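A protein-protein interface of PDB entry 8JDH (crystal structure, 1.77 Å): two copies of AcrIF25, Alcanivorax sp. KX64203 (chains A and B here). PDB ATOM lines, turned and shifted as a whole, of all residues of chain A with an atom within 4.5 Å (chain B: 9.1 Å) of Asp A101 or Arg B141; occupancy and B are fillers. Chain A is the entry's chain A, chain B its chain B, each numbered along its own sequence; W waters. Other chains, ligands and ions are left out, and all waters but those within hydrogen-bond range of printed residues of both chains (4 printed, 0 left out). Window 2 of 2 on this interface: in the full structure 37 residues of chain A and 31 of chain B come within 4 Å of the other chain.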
ATOM      1  N   ARG A  89       8.787  40.741  -6.546  1.00  0.00           N
ATOM      2  CA  ARG A  89       9.562  40.549  -7.765  1.00  0.00           C
ATOM      3  C   ARG A  89       8.672  40.108  -8.920  1.00  0.00           C
ATOM      4  O   ARG A  89       8.836  40.572 -10.058  1.00  0.00           O
ATOM      5  CB  ARG A  89      10.661  39.519  -7.493  1.00  0.00           C
ATOM      6  CG  ARG A  89      11.510  39.150  -8.689  1.00  0.00           C
ATOM      7  CD  ARG A  89      12.685  38.303  -8.234  1.00  0.00           C
ATOM      8  NE  ARG A  89      13.451  37.786  -9.368  1.00  0.00           N
ATOM      9  CZ  ARG A  89      13.649  36.498  -9.618  1.00  0.00           C
ATOM     10  NH1 ARG A  89      13.152  35.565  -8.811  1.00  0.00           N
ATOM     11  NH2 ARG A  89      14.360  36.141 -10.676  1.00  0.00           N
ATOM     12  N   ALA A  97       9.814  34.895 -18.070  1.00  0.00           N
ATOM     13  CA  ALA A  97      10.839  34.073 -17.429  1.00  0.00           C
ATOM     14  C   ALA A  97      11.076  34.514 -15.989  1.00  0.00           C
ATOM     15  O   ALA A  97      11.219  33.679 -15.083  1.00  0.00           O
ATOM     16  CB  ALA A  97      12.137  34.130 -18.228  1.00  0.00           C
ATOM     17  N   THR A  98      11.099  35.828 -15.759  1.00  0.00           N
ATOM     18  CA  THR A  98      11.252  36.333 -14.400  1.00  0.00           C
ATOM     19  C   THR A  98      10.009  36.059 -13.566  1.00  0.00           C
ATOM     20  O   THR A  98      10.117  35.669 -12.397  1.00  0.00           O
ATOM     21  CB  THR A  98      11.570  37.821 -14.435  1.00  0.00           C
ATOM     22  OG1 THR A  98      12.777  38.007 -15.186  1.00  0.00           O
ATOM     23  CG2 THR A  98      11.761  38.357 -13.018  1.00  0.00           C
ATOM     24  N   ARG A  99       8.819  36.258 -14.142  1.00  0.00           N
ATOM     25  CA  ARG A  99       7.598  35.903 -13.420  1.00  0.00           C
ATOM     26  C   ARG A  99       7.615  34.440 -12.996  1.00  0.00           C
ATOM     27  O   ARG A  99       7.257  34.115 -11.860  1.00  0.00           O
ATOM     28  CB  ARG A  99       6.368  36.199 -14.280  1.00  0.00           C
ATOM     29  CG  ARG A  99       6.061  37.685 -14.415  1.00  0.00           C
ATOM     30  CD  ARG A  99       4.942  37.908 -15.436  1.00  0.00           C
ATOM     31  NE  ARG A  99       4.806  39.314 -15.806  1.00  0.00           N
ATOM     32  CZ  ARG A  99       5.050  39.807 -17.016  1.00  0.00           C
ATOM     33  NH1 ARG A  99       5.434  39.008 -18.007  1.00  0.00           N
ATOM     34  NH2 ARG A  99       4.888  41.107 -17.240  1.00  0.00           N
ATOM     35  N   LEU A 100       8.021  33.542 -13.896  1.00  0.00           N
ATOM     36  CA  LEU A 100       8.056  32.118 -13.573  1.00  0.00           C
ATOM     37  C   LEU A 100       9.040  31.832 -12.451  1.00  0.00           C
ATOM     38  O   LEU A 100       8.727  31.110 -11.485  1.00  0.00           O
ATOM     39  CB  LEU A 100       8.421  31.315 -14.822  1.00  0.00           C
ATOM     40  CG  LEU A 100       8.649  29.824 -14.595  1.00  0.00           C
ATOM     41  CD1 LEU A 100       7.391  29.170 -14.068  1.00  0.00           C
ATOM     42  CD2 LEU A 100       9.121  29.138 -15.875  1.00  0.00           C
ATOM     43  N   ASP A 101      10.254  32.376 -12.567  1.00  0.00           N
ATOM     44  CA  ASP A 101      11.248  32.143 -11.528  1.00  0.00           C
ATOM     45  C   ASP A 101      10.753  32.642 -10.174  1.00  0.00           C
ATOM     46  O   ASP A 101      10.880  31.937  -9.161  1.00  0.00           O
ATOM     47  CB  ASP A 101      12.561  32.827 -11.906  1.00  0.00           C
ATOM     48  CG  ASP A 101      13.699  32.458 -10.971  1.00  0.00           C
ATOM     49  OD1 ASP A 101      14.084  31.267 -10.940  1.00  0.00           O
ATOM     50  OD2 ASP A 101      14.200  33.349 -10.259  1.00  0.00           O
ATOM     51  N   ALA A 102      10.136  33.835 -10.151  1.00  0.00           N
ATOM     52  CA  ALA A 102       9.670  34.418  -8.900  1.00  0.00           C
ATOM     53  C   ALA A 102       8.520  33.616  -8.302  1.00  0.00           C
ATOM     54  O   ALA A 102       8.462  33.434  -7.083  1.00  0.00           O
ATOM     55  CB  ALA A 102       9.244  35.869  -9.126  1.00  0.00           C
ATOM     56  N   ALA A 103       7.589  33.140  -9.137  1.00  0.00           N
ATOM     57  CA  ALA A 103       6.450  32.373  -8.622  1.00  0.00           C
ATOM     58  C   ALA A 103       6.903  31.054  -8.015  1.00  0.00           C
ATOM     59  O   ALA A 103       6.429  30.649  -6.930  1.00  0.00           O
ATOM     60  CB  ALA A 103       5.449  32.124  -9.748  1.00  0.00           C
ATOM     61  N   LEU A 104       7.874  30.396  -8.669  1.00  0.00           N
ATOM     62  CA  LEU A 104       8.405  29.147  -8.122  1.00  0.00           C
ATOM     63  C   LEU A 104       9.153  29.391  -6.817  1.00  0.00           C
ATOM     64  O   LEU A 104       8.989  28.648  -5.832  1.00  0.00           O
ATOM     65  CB  LEU A 104       9.329  28.490  -9.152  1.00  0.00           C
ATOM     66  CG  LEU A 104       8.679  27.990 -10.443  1.00  0.00           C
ATOM     67  CD1 LEU A 104       9.729  27.290 -11.296  1.00  0.00           C
ATOM     68  CD2 LEU A 104       7.513  27.065 -10.173  1.00  0.00           C
ATOM     69  N   TRP A 105       9.948  30.458  -6.778  1.00  0.00           N
ATOM     70  CA  TRP A 105      10.702  30.774  -5.579  1.00  0.00           C
ATOM     71  C   TRP A 105       9.780  31.194  -4.433  1.00  0.00           C
ATOM     72  O   TRP A 105      10.078  30.910  -3.270  1.00  0.00           O
ATOM     73  CB  TRP A 105      11.712  31.868  -5.923  1.00  0.00           C
ATOM     74  CG  TRP A 105      12.834  32.090  -4.959  1.00  0.00           C
ATOM     75  CD1 TRP A 105      12.910  31.698  -3.652  1.00  0.00           C
ATOM     76  CD2 TRP A 105      14.047  32.802  -5.237  1.00  0.00           C
ATOM     77  NE1 TRP A 105      14.107  32.120  -3.098  1.00  0.00           N
ATOM     78  CE2 TRP A 105      14.819  32.799  -4.055  1.00  0.00           C
ATOM     79  CE3 TRP A 105      14.557  33.436  -6.379  1.00  0.00           C
ATOM     80  CZ2 TRP A 105      16.076  33.404  -3.983  1.00  0.00           C
ATOM     81  CZ3 TRP A 105      15.808  34.036  -6.303  1.00  0.00           C
ATOM     82  CH2 TRP A 105      16.548  34.017  -5.112  1.00  0.00           C
ATOM     83  N   GLU A 108       8.788  28.139  -2.780  1.00  0.00           N
ATOM     84  CA  GLU A 108       9.925  27.687  -1.982  1.00  0.00           C
ATOM     85  C   GLU A 108       9.962  28.400  -0.626  1.00  0.00           C
ATOM     86  O   GLU A 108      10.299  27.795   0.408  1.00  0.00           O
ATOM     87  CB  GLU A 108      11.210  27.921  -2.785  1.00  0.00           C
ATOM     88  CG  GLU A 108      12.460  27.305  -2.222  1.00  0.00           C
ATOM     89  CD  GLU A 108      13.688  27.786  -2.983  1.00  0.00           C
ATOM     90  OE1 GLU A 108      13.643  27.810  -4.237  1.00  0.00           O
ATOM     91  OE2 GLU A 108      14.673  28.165  -2.328  1.00  0.00           O
ATOM     92  N   GLU A 146       4.276  20.997  -4.859  1.00  0.00           N
ATOM     93  CA  GLU A 146       5.259  21.633  -5.733  1.00  0.00           C
ATOM     94  C   GLU A 146       5.065  21.214  -7.192  1.00  0.00           C
ATOM     95  O   GLU A 146       5.126  22.054  -8.091  1.00  0.00           O
ATOM     96  CB  GLU A 146       6.671  21.306  -5.250  1.00  0.00           C
ATOM     97  CG  GLU A 146       7.773  21.960  -6.094  1.00  0.00           C
ATOM     98  CD  GLU A 146       9.169  21.755  -5.509  1.00  0.00           C
ATOM     99  OE1 GLU A 146       9.298  21.098  -4.459  1.00  0.00           O
ATOM    100  OE2 GLU A 146      10.146  22.222  -6.125  1.00  0.00           O
ATOM    101  N   ALA B  47       6.276  19.068  -1.170  1.00  0.00           N
ATOM    102  CA  ALA B  47       7.375  19.392  -2.060  1.00  0.00           C
ATOM    103  C   ALA B  47       7.758  18.164  -2.873  1.00  0.00           C
ATOM    104  O   ALA B  47       7.351  17.037  -2.569  1.00  0.00           O
ATOM    105  CB  ALA B  47       8.584  19.851  -1.254  1.00  0.00           C
ATOM    106  N   LEU B  48       8.546  18.390  -3.928  1.00  0.00           N
ATOM    107  CA  LEU B  48       9.098  17.263  -4.666  1.00  0.00           C
ATOM    108  C   LEU B  48       9.966  16.463  -3.710  1.00  0.00           C
ATOM    109  O   LEU B  48      10.646  17.034  -2.855  1.00  0.00           O
ATOM    110  CB  LEU B  48       9.935  17.746  -5.859  1.00  0.00           C
ATOM    111  CG  LEU B  48       9.251  18.512  -6.996  1.00  0.00           C
ATOM    112  CD1 LEU B  48      10.249  18.860  -8.096  1.00  0.00           C
ATOM    113  CD2 LEU B  48       8.082  17.715  -7.555  1.00  0.00           C
ATOM    114  N   VAL B  53      13.881  15.083  -7.242  1.00  0.00           N
ATOM    115  CA  VAL B  53      14.827  16.153  -7.568  1.00  0.00           C
ATOM    116  C   VAL B  53      16.084  15.573  -8.206  1.00  0.00           C
ATOM    117  O   VAL B  53      16.586  16.089  -9.210  1.00  0.00           O
ATOM    118  CB  VAL B  53      15.171  16.974  -6.316  1.00  0.00           C
ATOM    119  CG1 VAL B  53      16.384  17.886  -6.588  1.00  0.00           C
ATOM    120  CG2 VAL B  53      13.989  17.820  -5.915  1.00  0.00           C
ATOM    121  N   GLU B  56      15.500  14.236 -11.783  1.00  0.00           N
ATOM    122  CA  GLU B  56      15.401  15.335 -12.742  1.00  0.00           C
ATOM    123  C   GLU B  56      16.748  16.024 -12.952  1.00  0.00           C
ATOM    124  O   GLU B  56      17.096  16.396 -14.085  1.00  0.00           O
ATOM    125  CB  GLU B  56      14.354  16.342 -12.270  1.00  0.00           C
ATOM    126  CG  GLU B  56      12.940  15.773 -12.318  1.00  0.00           C
ATOM    127  CD  GLU B  56      11.876  16.812 -12.011  1.00  0.00           C
ATOM    128  OE1 GLU B  56      12.183  18.014 -12.117  1.00  0.00           O
ATOM    129  OE2 GLU B  56      10.731  16.427 -11.676  1.00  0.00           O
ATOM    130  N   MET B  60      18.922  16.531 -16.454  1.00  0.00           N
ATOM    131  CA  MET B  60      19.421  17.822 -16.931  1.00  0.00           C
ATOM    132  C   MET B  60      20.942  17.812 -17.102  1.00  0.00           C
ATOM    133  O   MET B  60      21.470  18.337 -18.089  1.00  0.00           O
ATOM    134  CB  MET B  60      19.009  18.938 -15.982  1.00  0.00           C
ATOM    135  CG  MET B  60      17.526  18.987 -15.792  1.00  0.00           C
ATOM    136  SD  MET B  60      17.080  20.292 -14.454  1.00  0.00           S
ATOM    137  CE  MET B  60      17.132  21.816 -15.556  1.00  0.00           C
ATOM    138  N   ARG B 107      23.874  18.084  -4.276  1.00  0.00           N
ATOM    139  CA  ARG B 107      23.716  19.533  -4.191  1.00  0.00           C
ATOM    140  C   ARG B 107      25.055  20.248  -4.361  1.00  0.00           C
ATOM    141  O   ARG B 107      25.112  21.321  -4.972  1.00  0.00           O
ATOM    142  CB  ARG B 107      23.072  19.924  -2.860  1.00  0.00           C
ATOM    143  CG  ARG B 107      22.696  21.391  -2.844  1.00  0.00           C
ATOM    144  CD  ARG B 107      22.373  21.909  -1.449  1.00  0.00           C
ATOM    145  NE  ARG B 107      22.378  23.370  -1.502  1.00  0.00           N
ATOM    146  CZ  ARG B 107      21.378  24.090  -1.996  1.00  0.00           C
ATOM    147  NH1 ARG B 107      20.281  23.483  -2.459  1.00  0.00           N
ATOM    148  NH2 ARG B 107      21.481  25.401  -2.041  1.00  0.00           N
ATOM    149  N   TYR B 110      25.580  20.562  -7.980  1.00  0.00           N
ATOM    150  CA  TYR B 110      24.797  21.686  -8.485  1.00  0.00           C
ATOM    151  C   TYR B 110      25.493  23.013  -8.189  1.00  0.00           C
ATOM    152  O   TYR B 110      25.529  23.908  -9.039  1.00  0.00           O
ATOM    153  CB  TYR B 110      23.384  21.654  -7.879  1.00  0.00           C
ATOM    154  CG  TYR B 110      22.789  23.023  -7.680  1.00  0.00           C
ATOM    155  CD1 TYR B 110      22.409  23.790  -8.760  1.00  0.00           C
ATOM    156  CD2 TYR B 110      22.612  23.546  -6.398  1.00  0.00           C
ATOM    157  CE1 TYR B 110      21.883  25.055  -8.589  1.00  0.00           C
ATOM    158  CE2 TYR B 110      22.081  24.806  -6.212  1.00  0.00           C
ATOM    159  CZ  TYR B 110      21.716  25.555  -7.315  1.00  0.00           C
ATOM    160  OH  TYR B 110      21.185  26.810  -7.131  1.00  0.00           O
ATOM    161  N   SER B 120      22.437  33.937 -13.591  1.00  0.00           N
ATOM    162  CA  SER B 120      21.241  34.035 -14.434  1.00  0.00           C
ATOM    163  C   SER B 120      21.547  33.712 -15.902  1.00  0.00           C
ATOM    164  O   SER B 120      21.036  34.362 -16.814  1.00  0.00           O
ATOM    165  CB  SER B 120      20.594  35.420 -14.309  1.00  0.00           C
ATOM    166  OG  SER B 120      19.924  35.566 -13.071  1.00  0.00           O
ATOM    167  N   TRP B 133      17.020  29.025 -18.472  1.00  0.00           N
ATOM    168  CA  TRP B 133      18.159  28.193 -18.841  1.00  0.00           C
ATOM    169  C   TRP B 133      17.957  26.767 -18.410  1.00  0.00           C
ATOM    170  O   TRP B 133      17.497  26.516 -17.296  1.00  0.00           O
ATOM    171  CB  TRP B 133      19.413  28.713 -18.226  1.00  0.00           C
ATOM    172  N   VAL B 134      18.329  25.827 -19.281  1.00  0.00           N
ATOM    173  CA  VAL B 134      18.367  24.435 -18.857  1.00  0.00           C
ATOM    174  C   VAL B 134      19.290  24.289 -17.655  1.00  0.00           C
ATOM    175  O   VAL B 134      19.050  23.474 -16.764  1.00  0.00           O
ATOM    176  CB  VAL B 134      18.778  23.520 -20.025  1.00  0.00           C
ATOM    177  CG1 VAL B 134      18.996  22.088 -19.539  1.00  0.00           C
ATOM    178  CG2 VAL B 134      17.708  23.539 -21.101  1.00  0.00           C
ATOM    179  N   THR B 135      20.334  25.103 -17.580  1.00  0.00           N
ATOM    180  CA  THR B 135      21.183  25.018 -16.399  1.00  0.00           C
ATOM    181  C   THR B 135      20.687  25.919 -15.266  1.00  0.00           C
ATOM    182  O   THR B 135      20.437  25.446 -14.153  1.00  0.00           O
ATOM    183  CB  THR B 135      22.626  25.354 -16.765  1.00  0.00           C
ATOM    184  N   ALA B 136      20.536  27.221 -15.532  1.00  0.00           N
ATOM    185  CA  ALA B 136      20.686  28.195 -14.447  1.00  0.00           C
ATOM    186  C   ALA B 136      19.426  28.407 -13.609  1.00  0.00           C
ATOM    187  O   ALA B 136      19.398  28.090 -12.416  1.00  0.00           O
ATOM    188  CB  ALA B 136      21.155  29.531 -15.033  1.00  0.00           C
ATOM    189  N   SER B 137      18.362  28.928 -14.220  1.00  0.00           N
ATOM    190  CA  SER B 137      17.129  29.135 -13.468  1.00  0.00           C
ATOM    191  C   SER B 137      16.552  27.803 -13.015  1.00  0.00           C
ATOM    192  O   SER B 137      16.335  27.574 -11.815  1.00  0.00           O
ATOM    193  CB  SER B 137      16.121  29.919 -14.312  1.00  0.00           C
ATOM    194  N   GLN B 138      16.345  26.897 -13.973  1.00  0.00           N
ATOM    195  CA  GLN B 138      15.686  25.628 -13.704  1.00  0.00           C
ATOM    196  C   GLN B 138      16.348  24.899 -12.542  1.00  0.00           C
ATOM    197  O   GLN B 138      15.707  24.611 -11.524  1.00  0.00           O
ATOM    198  CB  GLN B 138      15.685  24.781 -14.976  1.00  0.00           C
ATOM    199  N   MET B 139      17.651  24.649 -12.639  1.00  0.00           N
ATOM    200  CA  MET B 139      18.257  23.816 -11.609  1.00  0.00           C
ATOM    201  C   MET B 139      18.269  24.547 -10.274  1.00  0.00           C
ATOM    202  O   MET B 139      18.174  23.902  -9.227  1.00  0.00           O
ATOM    203  CB  MET B 139      19.663  23.346 -12.018  1.00  0.00           C
ATOM    204  CG  MET B 139      19.575  22.057 -12.841  1.00  0.00           C
ATOM    205  SD  MET B 139      21.158  20.930 -12.954  1.00  0.00           S
ATOM    206  CE  MET B 139      21.873  21.327 -11.258  1.00  0.00           C
ATOM    207  N   ALA B 140      18.318  25.886 -10.307  1.00  0.00           N
ATOM    208  CA  ALA B 140      18.295  26.632  -9.054  1.00  0.00           C
ATOM    209  C   ALA B 140      16.970  26.432  -8.330  1.00  0.00           C
ATOM    210  O   ALA B 140      16.940  26.281  -7.104  1.00  0.00           O
ATOM    211  CB  ALA B 140      18.541  28.115  -9.316  1.00  0.00           C
ATOM    212  N   ARG B 141      15.862  26.434  -9.081  1.00  0.00           N
ATOM    213  CA  ARG B 141      14.547  26.224  -8.477  1.00  0.00           C
ATOM    214  C   ARG B 141      14.340  24.770  -8.075  1.00  0.00           C
ATOM    215  O   ARG B 141      13.549  24.477  -7.171  1.00  0.00           O
ATOM    216  CB  ARG B 141      13.454  26.704  -9.434  1.00  0.00           C
ATOM    217  CG  ARG B 141      13.495  28.208  -9.695  1.00  0.00           C
ATOM    218  CD  ARG B 141      12.936  29.032  -8.523  1.00  0.00           C
ATOM    219  NE  ARG B 141      13.816  29.092  -7.352  1.00  0.00           N
ATOM    220  CZ  ARG B 141      14.898  29.855  -7.253  1.00  0.00           C
ATOM    221  NH1 ARG B 141      15.256  30.645  -8.255  1.00  0.00           N
ATOM    222  NH2 ARG B 141      15.625  29.829  -6.147  1.00  0.00           N
ATOM    223  N   LEU B 142      15.013  23.847  -8.755  1.00  0.00           N
ATOM    224  CA  LEU B 142      14.889  22.428  -8.437  1.00  0.00           C
ATOM    225  C   LEU B 142      15.535  22.115  -7.091  1.00  0.00           C
ATOM    226  O   LEU B 142      14.926  21.465  -6.228  1.00  0.00           O
ATOM    227  CB  LEU B 142      15.541  21.614  -9.561  1.00  0.00           C
ATOM    228  CG  LEU B 142      15.340  20.112  -9.666  1.00  0.00           C
ATOM    229  CD1 LEU B 142      13.862  19.781  -9.824  1.00  0.00           C
ATOM    230  CD2 LEU B 142      16.154  19.559 -10.850  1.00  0.00           C
ATOM    231  N   PHE B 143      16.768  22.582  -6.886  1.00  0.00           N
ATOM    232  CA  PHE B 143      17.466  22.306  -5.633  1.00  0.00           C
ATOM    233  C   PHE B 143      17.021  23.230  -4.501  1.00  0.00           C
ATOM    234  O   PHE B 143      17.139  22.869  -3.320  1.00  0.00           O
ATOM    235  CB  PHE B 143      18.975  22.410  -5.856  1.00  0.00           C
ATOM    236  CG  PHE B 143      19.577  21.155  -6.423  1.00  0.00           C
ATOM    237  CD1 PHE B 143      19.923  20.098  -5.588  1.00  0.00           C
ATOM    238  CD2 PHE B 143      19.751  21.017  -7.783  1.00  0.00           C
ATOM    239  CE1 PHE B 143      20.469  18.930  -6.107  1.00  0.00           C
ATOM    240  CE2 PHE B 143      20.307  19.847  -8.315  1.00  0.00           C
ATOM    241  CZ  PHE B 143      20.658  18.807  -7.462  1.00  0.00           C
ATOM    242  N   GLY B 144      16.566  24.438  -4.828  1.00  0.00           N
ATOM    243  CA  GLY B 144      16.157  25.379  -3.804  1.00  0.00           C
ATOM    244  C   GLY B 144      17.312  25.856  -2.933  1.00  0.00           C
ATOM    245  O   GLY B 144      18.482  25.647  -3.219  1.00  0.00           O
ATOM    246  N   GLY B 145      16.936  26.510  -1.831  1.00  0.00           N
ATOM    247  CA  GLY B 145      17.913  27.032  -0.902  1.00  0.00           C
ATOM    248  C   GLY B 145      18.530  25.960  -0.032  1.00  0.00           C
ATOM    249  O   GLY B 145      17.989  24.864   0.121  1.00  0.00           O
ATOM    250  N   GLU B 146      19.678  26.307   0.562  1.00  0.00           N
ATOM    251  CA  GLU B 146      20.455  25.335   1.332  1.00  0.00           C
ATOM    252  C   GLU B 146      19.729  24.892   2.602  1.00  0.00           C
ATOM    253  O   GLU B 146      19.661  23.691   2.912  1.00  0.00           O
ATOM    254  CB  GLU B 146      21.816  25.941   1.692  1.00  0.00           C
ATOM    255  CG  GLU B 146      22.733  24.979   2.435  1.00  0.00           C
ATOM    256  CD  GLU B 146      24.094  25.583   2.799  1.00  0.00           C
ATOM    257  OE1 GLU B 146      24.254  26.831   2.829  1.00  0.00           O
ATOM    258  OE2 GLU B 146      25.015  24.795   3.080  1.00  0.00           O
ATOM    259  N   LEU B 148      16.568  24.946   3.345  1.00  0.00           N
ATOM    260  CA  LEU B 148      15.409  24.136   2.994  1.00  0.00           C
ATOM    261  C   LEU B 148      15.828  22.754   2.503  1.00  0.00           C
ATOM    262  O   LEU B 148      15.201  21.751   2.855  1.00  0.00           O
ATOM    263  CB  LEU B 148      14.580  24.837   1.926  1.00  0.00           C
ATOM    264  CG  LEU B 148      13.446  23.979   1.346  1.00  0.00           C
ATOM    265  CD1 LEU B 148      12.418  23.616   2.436  1.00  0.00           C
ATOM    266  CD2 LEU B 148      12.777  24.703   0.174  1.00  0.00           C
ATOM    267  N   TRP B 149      16.872  22.685   1.671  1.00  0.00           N
ATOM    268  CA  TRP B 149      17.366  21.387   1.212  1.00  0.00           C
ATOM    269  C   TRP B 149      17.709  20.492   2.391  1.00  0.00           C
ATOM    270  O   TRP B 149      17.353  19.306   2.414  1.00  0.00           O
ATOM    271  CB  TRP B 149      18.599  21.588   0.325  1.00  0.00           C
ATOM    272  CG  TRP B 149      19.167  20.327  -0.263  1.00  0.00           C
ATOM    273  CD1 TRP B 149      20.315  19.682   0.108  1.00  0.00           C
ATOM    274  CD2 TRP B 149      18.603  19.560  -1.329  1.00  0.00           C
ATOM    275  NE1 TRP B 149      20.507  18.570  -0.683  1.00  0.00           N
ATOM    276  CE2 TRP B 149      19.469  18.474  -1.571  1.00  0.00           C
ATOM    277  CE3 TRP B 149      17.457  19.701  -2.121  1.00  0.00           C
ATOM    278  CZ2 TRP B 149      19.216  17.531  -2.558  1.00  0.00           C
ATOM    279  CZ3 TRP B 149      17.206  18.768  -3.094  1.00  0.00           C
ATOM    280  CH2 TRP B 149      18.080  17.689  -3.307  1.00  0.00           C
ATOM    281  N   ARG B 152      14.540  19.198   4.044  1.00  0.00           N
ATOM    282  CA  ARG B 152      13.913  18.168   3.210  1.00  0.00           C
ATOM    283  C   ARG B 152      14.684  16.863   3.293  1.00  0.00           C
ATOM    284  O   ARG B 152      14.088  15.776   3.368  1.00  0.00           O
ATOM    285  CB  ARG B 152      13.811  18.639   1.760  1.00  0.00           C
ATOM    286  CG  ARG B 152      12.891  19.827   1.600  1.00  0.00           C
ATOM    287  CD  ARG B 152      13.138  20.521   0.286  1.00  0.00           C
ATOM    288  NE  ARG B 152      12.649  19.738  -0.842  1.00  0.00           N
ATOM    289  CZ  ARG B 152      12.781  20.118  -2.105  1.00  0.00           C
ATOM    290  NH1 ARG B 152      13.393  21.261  -2.391  1.00  0.00           N
ATOM    291  NH2 ARG B 152      12.285  19.367  -3.075  1.00  0.00           N
HETATM  292  O   HOH W   1      12.410  21.025  -5.431  1.00  0.00           O
HETATM  293  O   HOH W   2      12.225  26.234  -5.816  1.00  0.00           O
HETATM  294  O   HOH W   3      16.472  29.296  -3.554  1.00  0.00           O
HETATM  295  O   HOH W   4      10.207  24.572  -7.739  1.00  0.00           O
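NH1 of Arg B141 lies within salt-bridge range of OD1 of Asp A101 (3.0 Å). OE1 of Glu A108 is in salt-bridge range of NE of Arg B141, at 3.4 Å. The side-chain carboxylate (OE2) of Glu A108 sits at hydrogen-bond distance from the backbone NH (N) of Gly B145. The side-chain carboxylate (OE1) of Glu A146 lies within hydrogen-bond range of the backbone NH (N) of Leu B48 (2.9 Å). OE1 of Glu A146 lies within salt-bridge range of NH2 of Arg B152, 3.7 Å away.
The guanidinium group of Arg A89 is in salt-bridge range of the side-chain carboxylate of Asp A101, at 2.8 Å. The backbone carbonyl oxygen (O) of Leu B48 sits at hydrogen-bond distance from the guanidinium group (NH2) of Arg B152 (2.9 Å). The backbone carbonyl oxygen of Gly B144 is in hydrogen-bond range of the guanidinium group of Arg B107, at 2.9 Å.
Leu A104 touches Arg B141 (CB to CD, 3.7 Å). Trp A105 touches Arg B141 (CE3 to NH1, 3.4 Å). Gly B144 touches Glu A108 (CA to OE2, 3.5 Å). Glu A108 touches Leu B148. CB of Ala B47 touches OE1 of Glu A146, at 3.5 Å.
No residue of chain B comes within 4 Å of Leu A100. No residue of chain B comes within 4 Å of Ala A102. Printed residues of chain B within 4 Å of Leu A104: Arg B141. Printed residues of chain B within 4 Å of Glu A146: Ala B47, Leu B48 and Arg B152. Printed residues of chain A within 4 Å of Ala B47: Glu A146. Printed residues of chain A within 4 Å of Leu B48: Glu A146. Val B53 touches none of the printed residues of chain A. Ala B140 touches none of the printed residues of chain A. Of chain A, only Asp A101 (3.0 Å), Leu A104 (3.7 Å), Trp A105 (3.4 Å) and Glu A108 (3.4 Å) come within 4 Å of Arg B141. Of the printed residues of chain A, Leu B148 touches Glu A108. The nearest residue of chain A that does not touch Arg B141 is Glu A146 (4.2 Å). The nearest printed residue of chain A that does not touch Arg B152 is Glu A108 (6.1 Å).
Of the 12 printed residues of chain A, 5 touch a printed residue of chain B. Printed residues of chain A that touch a printed residue of chain B: Asp A101, Leu A104, Trp A105, Glu A108 and Glu A146. Of the 25 printed residues of chain B, 7 touch a printed residue of chain A. Hydrophobic or aromatic side chains of chain B that line the printed part of chain A: Ala B47, Leu B48 and Leu B148.
Position printed for both chains: 146. Of the 10 pairs that touch across the chains among the printed residues, none has its exchanged pair printed and touching as well.
Water W3 lies within hydrogen-bond range of OE2 of Glu A108 (2.5 Å), NH2 of Arg B141 (2.8 Å) and N of Gly B145 (3.3 Å). Water W2 lies within hydrogen-bond range of the backbone carbonyl oxygen of Arg B141 (2.6 Å) and the side-chain carboxylate of Glu A108 (2.6 Å). Water W1 lies within hydrogen-bond range of the side-chain carboxylate of Glu A146 (2.7 Å), the backbone carbonyl oxygen of Leu B142 (2.7 Å) and the guanidinium group of Arg B152 (2.9 Å). Water W4 bridges OE2 of Glu A146 (2.9 Å) and O of Arg B141 (3.4 Å).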
